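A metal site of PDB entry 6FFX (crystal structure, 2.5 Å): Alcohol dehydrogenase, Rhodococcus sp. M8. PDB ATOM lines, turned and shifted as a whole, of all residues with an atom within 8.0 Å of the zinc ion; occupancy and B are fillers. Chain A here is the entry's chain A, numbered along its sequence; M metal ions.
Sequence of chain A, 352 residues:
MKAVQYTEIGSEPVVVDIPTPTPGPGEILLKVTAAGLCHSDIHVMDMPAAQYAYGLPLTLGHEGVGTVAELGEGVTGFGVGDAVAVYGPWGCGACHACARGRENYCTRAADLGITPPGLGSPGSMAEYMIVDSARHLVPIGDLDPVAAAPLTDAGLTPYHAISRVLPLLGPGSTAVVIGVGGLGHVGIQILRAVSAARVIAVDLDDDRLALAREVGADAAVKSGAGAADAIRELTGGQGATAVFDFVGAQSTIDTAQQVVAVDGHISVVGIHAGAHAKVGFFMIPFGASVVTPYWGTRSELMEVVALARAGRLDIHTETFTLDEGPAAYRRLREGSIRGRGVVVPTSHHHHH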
ATOM      1  N   TRP A  90      23.703 -21.169  27.702  1.00  0.00           N
ATOM      2  CA  TRP A  90      25.021 -20.611  27.433  1.00  0.00           C
ATOM      3  C   TRP A  90      25.910 -21.683  26.850  1.00  0.00           C
ATOM      4  O   TRP A  90      25.918 -22.825  27.334  1.00  0.00           O
ATOM      5  CB  TRP A  90      25.681 -20.053  28.700  1.00  0.00           C
ATOM      6  CG  TRP A  90      25.007 -18.884  29.356  1.00  0.00           C
ATOM      7  CD1 TRP A  90      24.000 -18.123  28.853  1.00  0.00           C
ATOM      8  CD2 TRP A  90      25.334 -18.329  30.637  1.00  0.00           C
ATOM      9  NE1 TRP A  90      23.649 -17.130  29.753  1.00  0.00           N
ATOM     10  CE2 TRP A  90      24.469 -17.233  30.847  1.00  0.00           C
ATOM     11  CE3 TRP A  90      26.283 -18.643  31.605  1.00  0.00           C
ATOM     12  CZ2 TRP A  90      24.498 -16.471  32.007  1.00  0.00           C
ATOM     13  CZ3 TRP A  90      26.332 -17.873  32.775  1.00  0.00           C
ATOM     14  CH2 TRP A  90      25.439 -16.813  32.963  1.00  0.00           C
ATOM     15  N   GLY A  91      26.669 -21.305  25.830  1.00  0.00           N
ATOM     16  CA  GLY A  91      27.666 -22.181  25.228  1.00  0.00           C
ATOM     17  C   GLY A  91      29.043 -21.559  25.318  1.00  0.00           C
ATOM     18  O   GLY A  91      29.213 -20.528  25.959  1.00  0.00           O
ATOM     19  N   CYS A  92      30.005 -22.204  24.644  1.00  0.00           N
ATOM     20  CA  CYS A  92      31.395 -21.764  24.664  1.00  0.00           C
ATOM     21  C   CYS A  92      31.668 -20.540  23.807  1.00  0.00           C
ATOM     22  O   CYS A  92      32.645 -19.835  24.039  1.00  0.00           O
ATOM     23  CB  CYS A  92      32.322 -22.907  24.254  1.00  0.00           C
ATOM     24  SG  CYS A  92      32.249 -23.345  22.511  1.00  0.00           S
ATOM     25  N   GLY A  93      30.832 -20.286  22.804  1.00  0.00           N
ATOM     26  CA  GLY A  93      30.948 -19.072  21.982  1.00  0.00           C
ATOM     27  C   GLY A  93      31.903 -19.182  20.796  1.00  0.00           C
ATOM     28  O   GLY A  93      31.900 -18.294  19.922  1.00  0.00           O
ATOM     29  N   ALA A  94      32.710 -20.259  20.747  1.00  0.00           N
ATOM     30  CA  ALA A  94      33.800 -20.420  19.789  1.00  0.00           C
ATOM     31  C   ALA A  94      33.601 -21.567  18.778  1.00  0.00           C
ATOM     32  O   ALA A  94      34.147 -21.506  17.677  1.00  0.00           O
ATOM     33  CB  ALA A  94      35.118 -20.631  20.522  1.00  0.00           C
ATOM     34  N   CYS A  95      32.828 -22.603  19.143  1.00  0.00           N
ATOM     35  CA  CYS A  95      32.637 -23.779  18.276  1.00  0.00           C
ATOM     36  C   CYS A  95      31.761 -23.433  17.076  1.00  0.00           C
ATOM     37  O   CYS A  95      31.124 -22.377  17.050  1.00  0.00           O
ATOM     38  CB  CYS A  95      32.011 -24.941  19.068  1.00  0.00           C
ATOM     39  SG  CYS A  95      30.219 -24.814  19.407  1.00  0.00           S
ATOM     40  N   HIS A  96      31.714 -24.343  16.099  1.00  0.00           N
ATOM     41  CA  HIS A  96      30.986 -24.133  14.841  1.00  0.00           C
ATOM     42  C   HIS A  96      29.520 -23.821  15.075  1.00  0.00           C
ATOM     43  O   HIS A  96      28.967 -22.903  14.456  1.00  0.00           O
ATOM     44  CB  HIS A  96      31.162 -25.355  13.928  1.00  0.00           C
ATOM     45  CG  HIS A  96      30.555 -25.186  12.562  1.00  0.00           C
ATOM     46  ND1 HIS A  96      29.388 -25.822  12.194  1.00  0.00           N
ATOM     47  CD2 HIS A  96      30.961 -24.477  11.485  1.00  0.00           C
ATOM     48  CE1 HIS A  96      29.110 -25.504  10.935  1.00  0.00           C
ATOM     49  NE2 HIS A  96      30.040 -24.689  10.489  1.00  0.00           N
ATOM     50  N   ALA A  97      28.895 -24.574  15.967  1.00  0.00           N
ATOM     51  CA  ALA A  97      27.499 -24.284  16.391  1.00  0.00           C
ATOM     52  C   ALA A  97      27.356 -22.918  17.104  1.00  0.00           C
ATOM     53  O   ALA A  97      26.428 -22.178  16.810  1.00  0.00           O
ATOM     54  CB  ALA A  97      26.964 -25.424  17.274  1.00  0.00           C
ATOM     55  N   CYS A  98      28.270 -22.589  18.023  1.00  0.00           N
ATOM     56  CA  CYS A  98      28.171 -21.326  18.777  1.00  0.00           C
ATOM     57  C   CYS A  98      28.390 -20.105  17.887  1.00  0.00           C
ATOM     58  O   CYS A  98      27.746 -19.081  18.075  1.00  0.00           O
ATOM     59  CB  CYS A  98      29.179 -21.274  19.935  1.00  0.00           C
ATOM     60  SG  CYS A  98      28.711 -22.295  21.364  1.00  0.00           S
ATOM     61  N   ALA A  99      29.282 -20.227  16.929  1.00  0.00           N
ATOM     62  CA  ALA A  99      29.520 -19.152  15.996  1.00  0.00           C
ATOM     63  C   ALA A  99      28.322 -18.846  15.120  1.00  0.00           C
ATOM     64  O   ALA A  99      28.242 -17.744  14.599  1.00  0.00           O
ATOM     65  CB  ALA A  99      30.720 -19.450  15.125  1.00  0.00           C
ATOM     66  N   ARG A 102      24.084 -20.871  17.724  1.00  0.00           N
ATOM     67  CA  ARG A 102      23.321 -22.046  18.120  1.00  0.00           C
ATOM     68  C   ARG A 102      23.929 -22.612  19.381  1.00  0.00           C
ATOM     69  O   ARG A 102      24.330 -23.767  19.417  1.00  0.00           O
ATOM     70  CB  ARG A 102      23.286 -23.070  16.980  1.00  0.00           C
ATOM     71  CG  ARG A 102      22.687 -22.516  15.701  1.00  0.00           C
ATOM     72  CD  ARG A 102      22.893 -23.405  14.476  1.00  0.00           C
ATOM     73  NE  ARG A 102      22.154 -24.661  14.552  1.00  0.00           N
ATOM     74  CZ  ARG A 102      20.852 -24.802  14.396  1.00  0.00           C
ATOM     75  NH1 ARG A 102      20.067 -23.747  14.211  1.00  0.00           N
ATOM     76  NH2 ARG A 102      20.305 -26.000  14.487  1.00  0.00           N
ATOM     77  N   GLU A 103      23.969 -21.798  20.438  1.00  0.00           N
ATOM     78  CA  GLU A 103      24.724 -22.158  21.650  1.00  0.00           C
ATOM     79  C   GLU A 103      24.004 -23.270  22.398  1.00  0.00           C
ATOM     80  O   GLU A 103      24.603 -23.994  23.194  1.00  0.00           O
ATOM     81  CB  GLU A 103      24.966 -20.942  22.558  1.00  0.00           C
ATOM     82  CG  GLU A 103      25.738 -19.803  21.890  1.00  0.00           C
ATOM     83  CD  GLU A 103      26.424 -18.844  22.869  1.00  0.00           C
ATOM     84  OE1 GLU A 103      26.396 -19.045  24.103  1.00  0.00           O
ATOM     85  OE2 GLU A 103      27.025 -17.867  22.380  1.00  0.00           O
ATOM     86  N   ASN A 104      22.703 -23.400  22.132  1.00  0.00           N
ATOM     87  CA  ASN A 104      21.920 -24.545  22.583  1.00  0.00           C
ATOM     88  C   ASN A 104      22.510 -25.880  22.140  1.00  0.00           C
ATOM     89  O   ASN A 104      22.410 -26.863  22.867  1.00  0.00           O
ATOM     90  CB  ASN A 104      20.445 -24.426  22.164  1.00  0.00           C
ATOM     91  CG  ASN A 104      20.267 -24.190  20.667  1.00  0.00           C
ATOM     92  OD1 ASN A 104      21.158 -23.671  20.005  1.00  0.00           O
ATOM     93  ND2 ASN A 104      19.102 -24.552  20.138  1.00  0.00           N
ATOM     94  N   TYR A 105      23.131 -25.915  20.961  1.00  0.00           N
ATOM     95  CA  TYR A 105      23.763 -27.125  20.432  1.00  0.00           C
ATOM     96  C   TYR A 105      25.302 -27.067  20.534  1.00  0.00           C
ATOM     97  O   TYR A 105      26.024 -27.680  19.707  1.00  0.00           O
ATOM     98  CB  TYR A 105      23.267 -27.399  19.002  1.00  0.00           C
ATOM     99  CG  TYR A 105      21.753 -27.633  18.898  1.00  0.00           C
ATOM    100  CD1 TYR A 105      21.070 -28.457  19.815  1.00  0.00           C
ATOM    101  CD2 TYR A 105      21.019 -27.039  17.900  1.00  0.00           C
ATOM    102  CE1 TYR A 105      19.709 -28.677  19.713  1.00  0.00           C
ATOM    103  CE2 TYR A 105      19.645 -27.247  17.785  1.00  0.00           C
ATOM    104  CZ  TYR A 105      18.993 -28.074  18.693  1.00  0.00           C
ATOM    105  OH  TYR A 105      17.627 -28.275  18.613  1.00  0.00           O
ATOM    106  N   CYS A 106      25.786 -26.377  21.557  1.00  0.00           N
ATOM    107  CA  CYS A 106      27.210 -26.304  21.832  1.00  0.00           C
ATOM    108  C   CYS A 106      27.699 -27.678  22.241  1.00  0.00           C
ATOM    109  O   CYS A 106      27.140 -28.280  23.146  1.00  0.00           O
ATOM    110  CB  CYS A 106      27.512 -25.311  22.958  1.00  0.00           C
ATOM    111  SG  CYS A 106      29.273 -25.177  23.295  1.00  0.00           S
ATOM    112  N   THR A 107      28.749 -28.146  21.575  1.00  0.00           N
ATOM    113  CA  THR A 107      29.360 -29.458  21.824  1.00  0.00           C
ATOM    114  C   THR A 107      30.332 -29.444  23.019  1.00  0.00           C
ATOM    115  O   THR A 107      30.519 -30.463  23.679  1.00  0.00           O
ATOM    116  CB  THR A 107      30.135 -29.918  20.557  1.00  0.00           C
ATOM    117  OG1 THR A 107      30.841 -28.799  19.998  1.00  0.00           O
ATOM    118  CG2 THR A 107      29.185 -30.466  19.481  1.00  0.00           C
ATOM    119  N   ARG A 108      30.923 -28.294  23.316  1.00  0.00           N
ATOM    120  CA  ARG A 108      32.039 -28.181  24.237  1.00  0.00           C
ATOM    121  C   ARG A 108      31.704 -27.508  25.581  1.00  0.00           C
ATOM    122  O   ARG A 108      32.581 -27.324  26.414  1.00  0.00           O
ATOM    123  CB  ARG A 108      33.175 -27.435  23.534  1.00  0.00           C
ATOM    124  CG  ARG A 108      33.574 -28.091  22.206  1.00  0.00           C
ATOM    125  CD  ARG A 108      34.469 -27.275  21.312  1.00  0.00           C
ATOM    126  NE  ARG A 108      35.679 -26.841  22.015  1.00  0.00           N
ATOM    127  CZ  ARG A 108      36.100 -25.582  22.202  1.00  0.00           C
ATOM    128  NH1 ARG A 108      37.224 -25.372  22.895  1.00  0.00           N
ATOM    129  NH2 ARG A 108      35.429 -24.533  21.712  1.00  0.00           N
ATOM    130  N   ALA A 109      30.430 -27.150  25.791  1.00  0.00           N
ATOM    131  CA  ALA A 109      29.999 -26.491  27.026  1.00  0.00           C
ATOM    132  C   ALA A 109      30.064 -27.437  28.210  1.00  0.00           C
ATOM    133  O   ALA A 109      30.482 -27.042  29.285  1.00  0.00           O
ATOM    134  CB  ALA A 109      28.578 -25.934  26.890  1.00  0.00           C
ATOM    135  N   LEU A 112      33.749 -27.930  29.368  1.00  0.00           N
ATOM    136  CA  LEU A 112      34.269 -26.662  29.924  1.00  0.00           C
ATOM    137  C   LEU A 112      33.567 -26.186  31.227  1.00  0.00           C
ATOM    138  O   LEU A 112      34.015 -25.214  31.850  1.00  0.00           O
ATOM    139  CB  LEU A 112      34.190 -25.532  28.880  1.00  0.00           C
ATOM    140  CG  LEU A 112      35.303 -25.490  27.822  1.00  0.00           C
ATOM    141  CD1 LEU A 112      34.867 -24.672  26.621  1.00  0.00           C
ATOM    142  CD2 LEU A 112      36.590 -24.912  28.394  1.00  0.00           C
ATOM    143  N   ILE A 114      30.453 -24.895  31.490  1.00  0.00           N
ATOM    144  CA  ILE A 114      29.542 -23.765  31.248  1.00  0.00           C
ATOM    145  C   ILE A 114      28.150 -24.340  31.379  1.00  0.00           C
ATOM    146  O   ILE A 114      27.786 -25.310  30.703  1.00  0.00           O
ATOM    147  CB  ILE A 114      29.744 -23.118  29.860  1.00  0.00           C
ATOM    148  CG1 ILE A 114      31.173 -22.535  29.747  1.00  0.00           C
ATOM    149  CG2 ILE A 114      28.703 -22.025  29.610  1.00  0.00           C
ATOM    150  CD1 ILE A 114      31.494 -21.933  28.376  1.00  0.00           C
ATOM    151  N   ARG A 135      27.055 -11.196  24.949  1.00  0.00           N
ATOM    152  CA  ARG A 135      26.343 -11.887  23.880  1.00  0.00           C
ATOM    153  C   ARG A 135      25.110 -12.647  24.371  1.00  0.00           C
ATOM    154  O   ARG A 135      24.289 -13.080  23.549  1.00  0.00           O
ATOM    155  CB  ARG A 135      27.307 -12.806  23.104  1.00  0.00           C
ATOM    156  CG  ARG A 135      27.660 -14.111  23.787  1.00  0.00           C
ATOM    157  CD  ARG A 135      28.702 -14.878  22.998  1.00  0.00           C
ATOM    158  NE  ARG A 135      28.870 -16.241  23.504  1.00  0.00           N
ATOM    159  CZ  ARG A 135      29.627 -16.583  24.552  1.00  0.00           C
ATOM    160  NH1 ARG A 135      30.300 -15.669  25.249  1.00  0.00           N
ATOM    161  NH2 ARG A 135      29.689 -17.860  24.933  1.00  0.00           N
HETATM  162 ZN    ZN M   1      30.216 -23.875  21.600  1.00  0.00          ZN
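The side-chain sulfur (SG) of Cys 106 sits close to the backbone NH (N) of Ala 109, at 3.4 Å. The guanidinium group (NH2) of Arg 108 lies close to the side-chain sulfur (SG) of Cys 92 (3.5 Å). The backbone NH of Ala 94 sits close to the side-chain sulfur of Cys 92, 3.6 Å away. The side-chain sulfur of Cys 98 lies close to the backbone NH of Gly 93 (3.3 Å). The side-chain sulfur (SG) of Cys 106 sits close to the backbone NH (N) of Arg 108, 3.5 Å away. SG of Cys 95 lies close to N of Ala 97 (3.7 Å).
Merely in contact with the zinc ion: Gly 93.
The zinc ion is bound by the side-chain sulfur (SG) of Cys 98 (2.2 Å), the side-chain sulfur (SG) of Cys 92 (2.3 Å), the side-chain sulfur (SG) of Cys 106 (2.3 Å) and the side-chain sulfur (SG) of Cys 95 (2.4 Å). The zinc ion has four donor atoms within binding distance.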
